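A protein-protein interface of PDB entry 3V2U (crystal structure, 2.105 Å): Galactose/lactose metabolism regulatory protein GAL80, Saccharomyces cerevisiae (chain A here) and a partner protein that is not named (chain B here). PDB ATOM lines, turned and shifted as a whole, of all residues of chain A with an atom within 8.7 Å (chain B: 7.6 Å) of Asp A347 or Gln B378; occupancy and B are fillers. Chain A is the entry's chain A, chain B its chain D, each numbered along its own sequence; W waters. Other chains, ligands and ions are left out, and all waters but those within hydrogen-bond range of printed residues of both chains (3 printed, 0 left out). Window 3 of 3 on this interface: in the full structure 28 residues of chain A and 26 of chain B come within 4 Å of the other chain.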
ATOM      1  N   GLY A 326      24.760  26.370  27.961  1.00  0.00           N
ATOM      2  CA  GLY A 326      23.731  26.560  28.975  1.00  0.00           C
ATOM      3  C   GLY A 326      22.298  26.471  28.453  1.00  0.00           C
ATOM      4  O   GLY A 326      22.031  25.785  27.461  1.00  0.00           O
ATOM      5  N   THR A 327      21.378  27.178  29.117  1.00  0.00           N
ATOM      6  CA  THR A 327      19.950  27.177  28.750  1.00  0.00           C
ATOM      7  C   THR A 327      19.200  28.398  29.295  1.00  0.00           C
ATOM      8  O   THR A 327      19.608  28.991  30.294  1.00  0.00           O
ATOM      9  CB  THR A 327      19.230  25.908  29.262  1.00  0.00           C
ATOM     10  OG1 THR A 327      17.854  25.939  28.860  1.00  0.00           O
ATOM     11  CG2 THR A 327      19.295  25.826  30.776  1.00  0.00           C
ATOM     12  N   ARG A 328      18.102  28.775  28.644  1.00  0.00           N
ATOM     13  CA  ARG A 328      17.234  29.818  29.185  1.00  0.00           C
ATOM     14  C   ARG A 328      15.925  29.202  29.688  1.00  0.00           C
ATOM     15  O   ARG A 328      14.920  29.892  29.876  1.00  0.00           O
ATOM     16  CB  ARG A 328      16.968  30.920  28.150  1.00  0.00           C
ATOM     17  CG  ARG A 328      18.202  31.677  27.709  1.00  0.00           C
ATOM     18  CD  ARG A 328      17.856  32.998  27.018  1.00  0.00           C
ATOM     19  NE  ARG A 328      16.849  32.830  25.978  1.00  0.00           N
ATOM     20  CZ  ARG A 328      16.212  33.834  25.378  1.00  0.00           C
ATOM     21  NH1 ARG A 328      16.474  35.090  25.707  1.00  0.00           N
ATOM     22  NH2 ARG A 328      15.308  33.583  24.446  1.00  0.00           N
ATOM     23  N   ALA A 329      15.946  27.893  29.903  1.00  0.00           N
ATOM     24  CA  ALA A 329      14.784  27.196  30.431  1.00  0.00           C
ATOM     25  C   ALA A 329      14.705  27.353  31.950  1.00  0.00           C
ATOM     26  O   ALA A 329      13.712  27.856  32.485  1.00  0.00           O
ATOM     27  CB  ALA A 329      14.828  25.726  30.039  1.00  0.00           C
ATOM     28  N   PRO A 344      14.976  30.240  17.033  1.00  0.00           N
ATOM     29  CA  PRO A 344      15.317  28.830  16.832  1.00  0.00           C
ATOM     30  C   PRO A 344      14.520  27.912  17.762  1.00  0.00           C
ATOM     31  O   PRO A 344      14.396  28.214  18.954  1.00  0.00           O
ATOM     32  CB  PRO A 344      16.790  28.801  17.216  1.00  0.00           C
ATOM     33  CG  PRO A 344      16.867  29.805  18.353  1.00  0.00           C
ATOM     34  CD  PRO A 344      15.776  30.839  18.115  1.00  0.00           C
ATOM     35  N   GLY A 345      14.012  26.803  17.227  1.00  0.00           N
ATOM     36  CA  GLY A 345      13.131  25.910  17.969  1.00  0.00           C
ATOM     37  C   GLY A 345      13.816  24.823  18.789  1.00  0.00           C
ATOM     38  O   GLY A 345      14.110  23.732  18.284  1.00  0.00           O
ATOM     39  N   TYR A 346      14.035  25.107  20.071  1.00  0.00           N
ATOM     40  CA  TYR A 346      14.816  24.220  20.930  1.00  0.00           C
ATOM     41  C   TYR A 346      13.999  23.395  21.930  1.00  0.00           C
ATOM     42  O   TYR A 346      12.839  23.693  22.217  1.00  0.00           O
ATOM     43  CB  TYR A 346      15.896  25.017  21.665  1.00  0.00           C
ATOM     44  CG  TYR A 346      17.045  25.443  20.770  1.00  0.00           C
ATOM     45  CD1 TYR A 346      17.481  24.625  19.729  1.00  0.00           C
ATOM     46  CD2 TYR A 346      17.689  26.660  20.960  1.00  0.00           C
ATOM     47  CE1 TYR A 346      18.528  25.006  18.908  1.00  0.00           C
ATOM     48  CE2 TYR A 346      18.739  27.051  20.140  1.00  0.00           C
ATOM     49  CZ  TYR A 346      19.151  26.219  19.117  1.00  0.00           C
ATOM     50  OH  TYR A 346      20.190  26.596  18.297  1.00  0.00           O
ATOM     51  N   ASP A 347      14.635  22.349  22.448  1.00  0.00           N
ATOM     52  CA  ASP A 347      14.042  21.457  23.437  1.00  0.00           C
ATOM     53  C   ASP A 347      14.348  21.993  24.833  1.00  0.00           C
ATOM     54  O   ASP A 347      15.491  22.341  25.138  1.00  0.00           O
ATOM     55  CB  ASP A 347      14.606  20.041  23.259  1.00  0.00           C
ATOM     56  CG  ASP A 347      14.122  19.066  24.324  1.00  0.00           C
ATOM     57  OD1 ASP A 347      14.030  19.450  25.511  1.00  0.00           O
ATOM     58  OD2 ASP A 347      13.849  17.898  23.972  1.00  0.00           O
ATOM     59  N   ALA A 348      13.325  22.047  25.680  1.00  0.00           N
ATOM     60  CA  ALA A 348      13.433  22.678  26.995  1.00  0.00           C
ATOM     61  C   ALA A 348      14.471  22.049  27.934  1.00  0.00           C
ATOM     62  O   ALA A 348      15.120  22.754  28.703  1.00  0.00           O
ATOM     63  CB  ALA A 348      12.058  22.729  27.669  1.00  0.00           C
ATOM     64  N   GLY A 349      14.634  20.730  27.873  1.00  0.00           N
ATOM     65  CA  GLY A 349      15.522  20.052  28.804  1.00  0.00           C
ATOM     66  C   GLY A 349      16.912  19.715  28.292  1.00  0.00           C
ATOM     67  O   GLY A 349      17.528  18.752  28.755  1.00  0.00           O
ATOM     68  N   LYS A 350      17.418  20.506  27.350  1.00  0.00           N
ATOM     69  CA  LYS A 350      18.711  20.214  26.737  1.00  0.00           C
ATOM     70  C   LYS A 350      19.603  21.447  26.651  1.00  0.00           C
ATOM     71  O   LYS A 350      19.161  22.530  26.256  1.00  0.00           O
ATOM     72  CB  LYS A 350      18.512  19.585  25.354  1.00  0.00           C
ATOM     73  CG  LYS A 350      17.786  18.238  25.398  1.00  0.00           C
ATOM     74  CD  LYS A 350      17.340  17.778  24.013  1.00  0.00           C
ATOM     75  CE  LYS A 350      18.446  17.044  23.259  1.00  0.00           C
ATOM     76  NZ  LYS A 350      18.540  15.588  23.596  1.00  0.00           N
ATOM     77  N   GLU A 351      20.862  21.285  27.030  1.00  0.00           N
ATOM     78  CA  GLU A 351      21.817  22.386  26.947  1.00  0.00           C
ATOM     79  C   GLU A 351      22.082  22.773  25.499  1.00  0.00           C
ATOM     80  O   GLU A 351      22.112  21.928  24.602  1.00  0.00           O
ATOM     81  CB  GLU A 351      23.128  22.025  27.647  1.00  0.00           C
ATOM     82  CG  GLU A 351      22.982  21.800  29.143  1.00  0.00           C
ATOM     83  CD  GLU A 351      23.794  22.784  29.975  1.00  0.00           C
ATOM     84  OE1 GLU A 351      25.009  22.932  29.717  1.00  0.00           O
ATOM     85  OE2 GLU A 351      23.215  23.409  30.888  1.00  0.00           O
ATOM     86  N   ILE A 352      22.238  24.070  25.281  1.00  0.00           N
ATOM     87  CA  ILE A 352      22.648  24.598  24.002  1.00  0.00           C
ATOM     88  C   ILE A 352      24.164  24.780  24.037  1.00  0.00           C
ATOM     89  O   ILE A 352      24.705  25.289  25.007  1.00  0.00           O
ATOM     90  CB  ILE A 352      22.010  25.964  23.767  1.00  0.00           C
ATOM     91  CG1 ILE A 352      20.487  25.828  23.629  1.00  0.00           C
ATOM     92  CG2 ILE A 352      22.646  26.677  22.567  1.00  0.00           C
ATOM     93  CD1 ILE A 352      19.767  27.169  23.746  1.00  0.00           C
ATOM     94  N   MET A 353      24.838  24.358  22.979  1.00  0.00           N
ATOM     95  CA  MET A 353      26.278  24.532  22.859  1.00  0.00           C
ATOM     96  C   MET A 353      26.527  25.558  21.748  1.00  0.00           C
ATOM     97  O   MET A 353      25.917  25.490  20.692  1.00  0.00           O
ATOM     98  CB  MET A 353      26.922  23.196  22.478  1.00  0.00           C
ATOM     99  CG  MET A 353      28.405  23.307  22.105  1.00  0.00           C
ATOM    100  SD  MET A 353      29.485  23.295  23.547  1.00  0.00           S
ATOM    101  CE  MET A 353      30.708  24.524  23.102  1.00  0.00           C
ATOM    102  N   GLU A 354      27.406  26.519  21.993  1.00  0.00           N
ATOM    103  CA  GLU A 354      27.840  27.398  20.925  1.00  0.00           C
ATOM    104  C   GLU A 354      29.341  27.615  20.951  1.00  0.00           C
ATOM    105  O   GLU A 354      29.946  27.799  22.012  1.00  0.00           O
ATOM    106  CB  GLU A 354      27.129  28.748  20.993  1.00  0.00           C
ATOM    107  CG  GLU A 354      27.681  29.761  19.997  1.00  0.00           C
ATOM    108  CD  GLU A 354      26.870  31.053  19.952  1.00  0.00           C
ATOM    109  OE1 GLU A 354      25.802  31.127  20.583  1.00  0.00           O
ATOM    110  OE2 GLU A 354      27.299  32.001  19.280  1.00  0.00           O
ATOM    111  N   LEU B 268      25.872  24.775  10.096  1.00  0.00           N
ATOM    112  CA  LEU B 268      25.610  23.637  10.973  1.00  0.00           C
ATOM    113  C   LEU B 268      25.452  22.377  10.131  1.00  0.00           C
ATOM    114  O   LEU B 268      25.991  21.331  10.472  1.00  0.00           O
ATOM    115  CB  LEU B 268      24.360  23.880  11.837  1.00  0.00           C
ATOM    116  CG  LEU B 268      23.946  22.696  12.727  1.00  0.00           C
ATOM    117  CD1 LEU B 268      25.106  22.221  13.656  1.00  0.00           C
ATOM    118  CD2 LEU B 268      22.680  23.019  13.522  1.00  0.00           C
ATOM    119  N   SER B 347      16.856  11.036  17.453  1.00  0.00           N
ATOM    120  CA  SER B 347      16.751  12.271  18.236  1.00  0.00           C
ATOM    121  C   SER B 347      18.011  13.145  18.128  1.00  0.00           C
ATOM    122  O   SER B 347      17.987  14.319  18.472  1.00  0.00           O
ATOM    123  CB  SER B 347      16.441  11.959  19.705  1.00  0.00           C
ATOM    124  OG  SER B 347      17.509  11.256  20.318  1.00  0.00           O
ATOM    125  N   GLY B 348      19.107  12.573  17.639  1.00  0.00           N
ATOM    126  CA  GLY B 348      20.323  13.344  17.447  1.00  0.00           C
ATOM    127  C   GLY B 348      21.394  13.125  18.509  1.00  0.00           C
ATOM    128  O   GLY B 348      21.136  12.524  19.552  1.00  0.00           O
ATOM    129  N   PHE B 349      22.600  13.619  18.241  1.00  0.00           N
ATOM    130  CA  PHE B 349      23.748  13.397  19.127  1.00  0.00           C
ATOM    131  C   PHE B 349      24.099  14.685  19.861  1.00  0.00           C
ATOM    132  O   PHE B 349      24.340  15.716  19.232  1.00  0.00           O
ATOM    133  CB  PHE B 349      24.976  12.951  18.322  1.00  0.00           C
ATOM    134  CG  PHE B 349      24.876  11.564  17.742  1.00  0.00           C
ATOM    135  CD1 PHE B 349      24.039  11.297  16.662  1.00  0.00           C
ATOM    136  CD2 PHE B 349      25.649  10.534  18.258  1.00  0.00           C
ATOM    137  CE1 PHE B 349      23.954  10.015  16.125  1.00  0.00           C
ATOM    138  CE2 PHE B 349      25.584   9.241  17.728  1.00  0.00           C
ATOM    139  CZ  PHE B 349      24.728   8.982  16.655  1.00  0.00           C
ATOM    140  N   THR B 350      24.122  14.647  21.190  1.00  0.00           N
ATOM    141  CA  THR B 350      24.639  15.784  21.939  1.00  0.00           C
ATOM    142  C   THR B 350      26.140  15.878  21.661  1.00  0.00           C
ATOM    143  O   THR B 350      26.730  14.984  21.047  1.00  0.00           O
ATOM    144  CB  THR B 350      24.465  15.610  23.442  1.00  0.00           C
ATOM    145  OG1 THR B 350      25.122  14.402  23.839  1.00  0.00           O
ATOM    146  CG2 THR B 350      22.974  15.558  23.826  1.00  0.00           C
ATOM    147  N   VAL B 351      26.769  16.950  22.114  1.00  0.00           N
ATOM    148  CA  VAL B 351      28.206  17.066  21.904  1.00  0.00           C
ATOM    149  C   VAL B 351      28.962  15.887  22.575  1.00  0.00           C
ATOM    150  O   VAL B 351      29.945  15.377  22.029  1.00  0.00           O
ATOM    151  CB  VAL B 351      28.741  18.459  22.338  1.00  0.00           C
ATOM    152  CG1 VAL B 351      28.827  18.561  23.857  1.00  0.00           C
ATOM    153  CG2 VAL B 351      30.091  18.754  21.682  1.00  0.00           C
ATOM    154  N   HIS B 352      28.477  15.429  23.730  1.00  0.00           N
ATOM    155  CA  HIS B 352      29.120  14.314  24.442  1.00  0.00           C
ATOM    156  C   HIS B 352      28.986  13.006  23.667  1.00  0.00           C
ATOM    157  O   HIS B 352      29.945  12.237  23.544  1.00  0.00           O
ATOM    158  CB  HIS B 352      28.541  14.149  25.854  1.00  0.00           C
ATOM    159  CG  HIS B 352      29.115  15.099  26.864  1.00  0.00           C
ATOM    160  ND1 HIS B 352      28.880  16.459  26.832  1.00  0.00           N
ATOM    161  CD2 HIS B 352      29.903  14.882  27.944  1.00  0.00           C
ATOM    162  CE1 HIS B 352      29.505  17.037  27.841  1.00  0.00           C
ATOM    163  NE2 HIS B 352      30.134  16.103  28.531  1.00  0.00           N
ATOM    164  N   GLU B 353      27.795  12.767  23.131  1.00  0.00           N
ATOM    165  CA  GLU B 353      27.541  11.567  22.359  1.00  0.00           C
ATOM    166  C   GLU B 353      28.307  11.553  21.042  1.00  0.00           C
ATOM    167  O   GLU B 353      28.790  10.511  20.619  1.00  0.00           O
ATOM    168  CB  GLU B 353      26.041  11.412  22.126  1.00  0.00           C
ATOM    169  CG  GLU B 353      25.271  11.245  23.432  1.00  0.00           C
ATOM    170  CD  GLU B 353      23.769  11.348  23.240  1.00  0.00           C
ATOM    171  OE1 GLU B 353      23.319  11.995  22.261  1.00  0.00           O
ATOM    172  OE2 GLU B 353      23.040  10.780  24.079  1.00  0.00           O
ATOM    173  N   ARG B 376      25.926  26.790  16.519  1.00  0.00           N
ATOM    174  CA  ARG B 376      25.060  26.769  17.697  1.00  0.00           C
ATOM    175  C   ARG B 376      24.081  25.603  17.508  1.00  0.00           C
ATOM    176  O   ARG B 376      23.491  25.468  16.442  1.00  0.00           O
ATOM    177  CB  ARG B 376      24.320  28.122  17.804  1.00  0.00           C
ATOM    178  CG  ARG B 376      23.298  28.267  18.927  1.00  0.00           C
ATOM    179  CD  ARG B 376      22.570  29.641  18.835  1.00  0.00           C
ATOM    180  NE  ARG B 376      23.474  30.681  18.337  1.00  0.00           N
ATOM    181  CZ  ARG B 376      23.185  31.554  17.373  1.00  0.00           C
ATOM    182  NH1 ARG B 376      21.991  31.554  16.797  1.00  0.00           N
ATOM    183  NH2 ARG B 376      24.097  32.442  16.990  1.00  0.00           N
ATOM    184  N   PHE B 377      23.916  24.754  18.521  1.00  0.00           N
ATOM    185  CA  PHE B 377      23.064  23.566  18.394  1.00  0.00           C
ATOM    186  C   PHE B 377      22.808  22.916  19.749  1.00  0.00           C
ATOM    187  O   PHE B 377      23.548  23.168  20.705  1.00  0.00           O
ATOM    188  CB  PHE B 377      23.719  22.526  17.463  1.00  0.00           C
ATOM    189  CG  PHE B 377      24.995  21.934  18.019  1.00  0.00           C
ATOM    190  CD1 PHE B 377      24.976  20.752  18.743  1.00  0.00           C
ATOM    191  CD2 PHE B 377      26.207  22.584  17.855  1.00  0.00           C
ATOM    192  CE1 PHE B 377      26.147  20.217  19.266  1.00  0.00           C
ATOM    193  CE2 PHE B 377      27.371  22.060  18.371  1.00  0.00           C
ATOM    194  CZ  PHE B 377      27.341  20.863  19.081  1.00  0.00           C
ATOM    195  N   GLN B 378      21.766  22.083  19.829  1.00  0.00           N
ATOM    196  CA  GLN B 378      21.574  21.187  20.975  1.00  0.00           C
ATOM    197  C   GLN B 378      22.019  19.766  20.628  1.00  0.00           C
ATOM    198  O   GLN B 378      22.618  19.063  21.453  1.00  0.00           O
ATOM    199  CB  GLN B 378      20.105  21.170  21.421  1.00  0.00           C
ATOM    200  CG  GLN B 378      19.613  22.515  21.966  1.00  0.00           C
ATOM    201  CD  GLN B 378      18.175  22.456  22.444  1.00  0.00           C
ATOM    202  OE1 GLN B 378      17.294  21.979  21.736  1.00  0.00           O
ATOM    203  NE2 GLN B 378      17.939  22.920  23.660  1.00  0.00           N
ATOM    204  N   VAL B 379      21.694  19.344  19.408  1.00  0.00           N
ATOM    205  CA  VAL B 379      22.058  18.035  18.914  1.00  0.00           C
ATOM    206  C   VAL B 379      22.563  18.144  17.482  1.00  0.00           C
ATOM    207  O   VAL B 379      22.332  19.149  16.804  1.00  0.00           O
ATOM    208  CB  VAL B 379      20.872  17.037  18.978  1.00  0.00           C
ATOM    209  CG1 VAL B 379      20.479  16.767  20.434  1.00  0.00           C
ATOM    210  CG2 VAL B 379      19.674  17.557  18.181  1.00  0.00           C
ATOM    211  N   LEU B 380      23.288  17.121  17.048  1.00  0.00           N
ATOM    212  CA  LEU B 380      23.686  17.000  15.660  1.00  0.00           C
ATOM    213  C   LEU B 380      22.963  15.777  15.107  1.00  0.00           C
ATOM    214  O   LEU B 380      23.050  14.694  15.683  1.00  0.00           O
ATOM    215  CB  LEU B 380      25.208  16.824  15.558  1.00  0.00           C
ATOM    216  CG  LEU B 380      26.067  17.906  16.207  1.00  0.00           C
ATOM    217  CD1 LEU B 380      27.552  17.500  16.226  1.00  0.00           C
ATOM    218  CD2 LEU B 380      25.858  19.253  15.495  1.00  0.00           C
HETATM  219  O   HOH W   1      22.301  19.154  24.019  1.00  0.00           O
HETATM  220  O   HOH W   2      20.232  13.045  22.275  1.00  0.00           O
HETATM  221  O   HOH W   3      20.897  24.855  16.171  1.00  0.00           O
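Water W1 bridges O of Gln B378 and O of Glu A351.
Water W3 lies within hydrogen-bond range of O of Arg B376 (2.7 Å) and OH of Tyr A346 (2.8 Å).
Water W2 lies within hydrogen-bond range of the backbone carbonyl oxygen (O) of Gly B348 (2.9 Å), the side-chain carboxylate (OE1) of Glu B353 (3.3 Å) and the side-chain amino group (NZ) of Lys A350 (3.3 Å).
The backbone NH (N) of Met A353 is in hydrogen-bond range of the backbone carbonyl oxygen (O) of Phe B377.
The side-chain amide nitrogen of Gln B378 sits at hydrogen-bond distance from the backbone carbonyl oxygen of Lys A350 (2.9 Å).
N of Asp A347 is in hydrogen-bond range of OE1 of Gln B378 (2.8 Å).
OE1 of Glu A354 lies within salt-bridge range of NE of Arg B376.
Printed residues of chain A that touch a printed residue of chain B: Tyr A346, Asp A347, Lys A350, Glu A351, Ile A352, Met A353 and Glu A354.
Hydrophobic or aromatic side chains of chain A within 4 Å of the printed part of chain B: Tyr A346, Ile A352 and Met A353.
Hydrophobic or aromatic side chains of chain B within 4 Å of the printed part of chain A: Val B379.
Among the printed residues, Asp or Glu carboxylates within 4 Å of a Lys or Arg side-chain nitrogen of the other chain: Glu A354 with Arg B376 (3.3 Å).
Asp A347 touches one residue of chain B.
Printed residues of chain A within 4 Å of Gln B378: Tyr A346 (3.3 Å), Asp A347 (2.8 Å), Lys A350 (2.9 Å), Glu A351 (3.7 Å) and Ile A352 (3.8 Å).
Of the printed residues of chain B, Met A353 touches Arg B376 and Phe B377.
Printed residues of chain B within 4 Å of Tyr A346: Arg B376 and Gln B378.
Of the printed residues of chain B, Lys A350 touches Gln B378 (2.9 Å) and Val B379 (3.5 Å).
Of the printed residues of chain B, Glu A354 touches Arg B376.
Of the printed residues of chain B, Ile A352 touches Phe B377 (3.7 Å) and Gln B378 (3.8 Å).
Gly A326 touches none of the printed residues of chain B.
The nearest residue of chain A that does not touch Gln B378 is Met A353 (5.0 Å).
Among the printed residues, merely in contact across the chains: Tyr A346 with Gln B378, Met A353 with Arg B376, Lys A350 with Val B379, Tyr A346 with Arg B376, Glu A351 with Gln B378, Ile A352 with Phe B377 and Ile A352 with Gln B378.
O of Gly A326 sits at hydrogen-bond distance from N of Ile A352, at 2.8 Å.
The side-chain carboxylate (OD1) of Asp A347 is in hydrogen-bond range of the backbone NH (N) of Gly A349.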
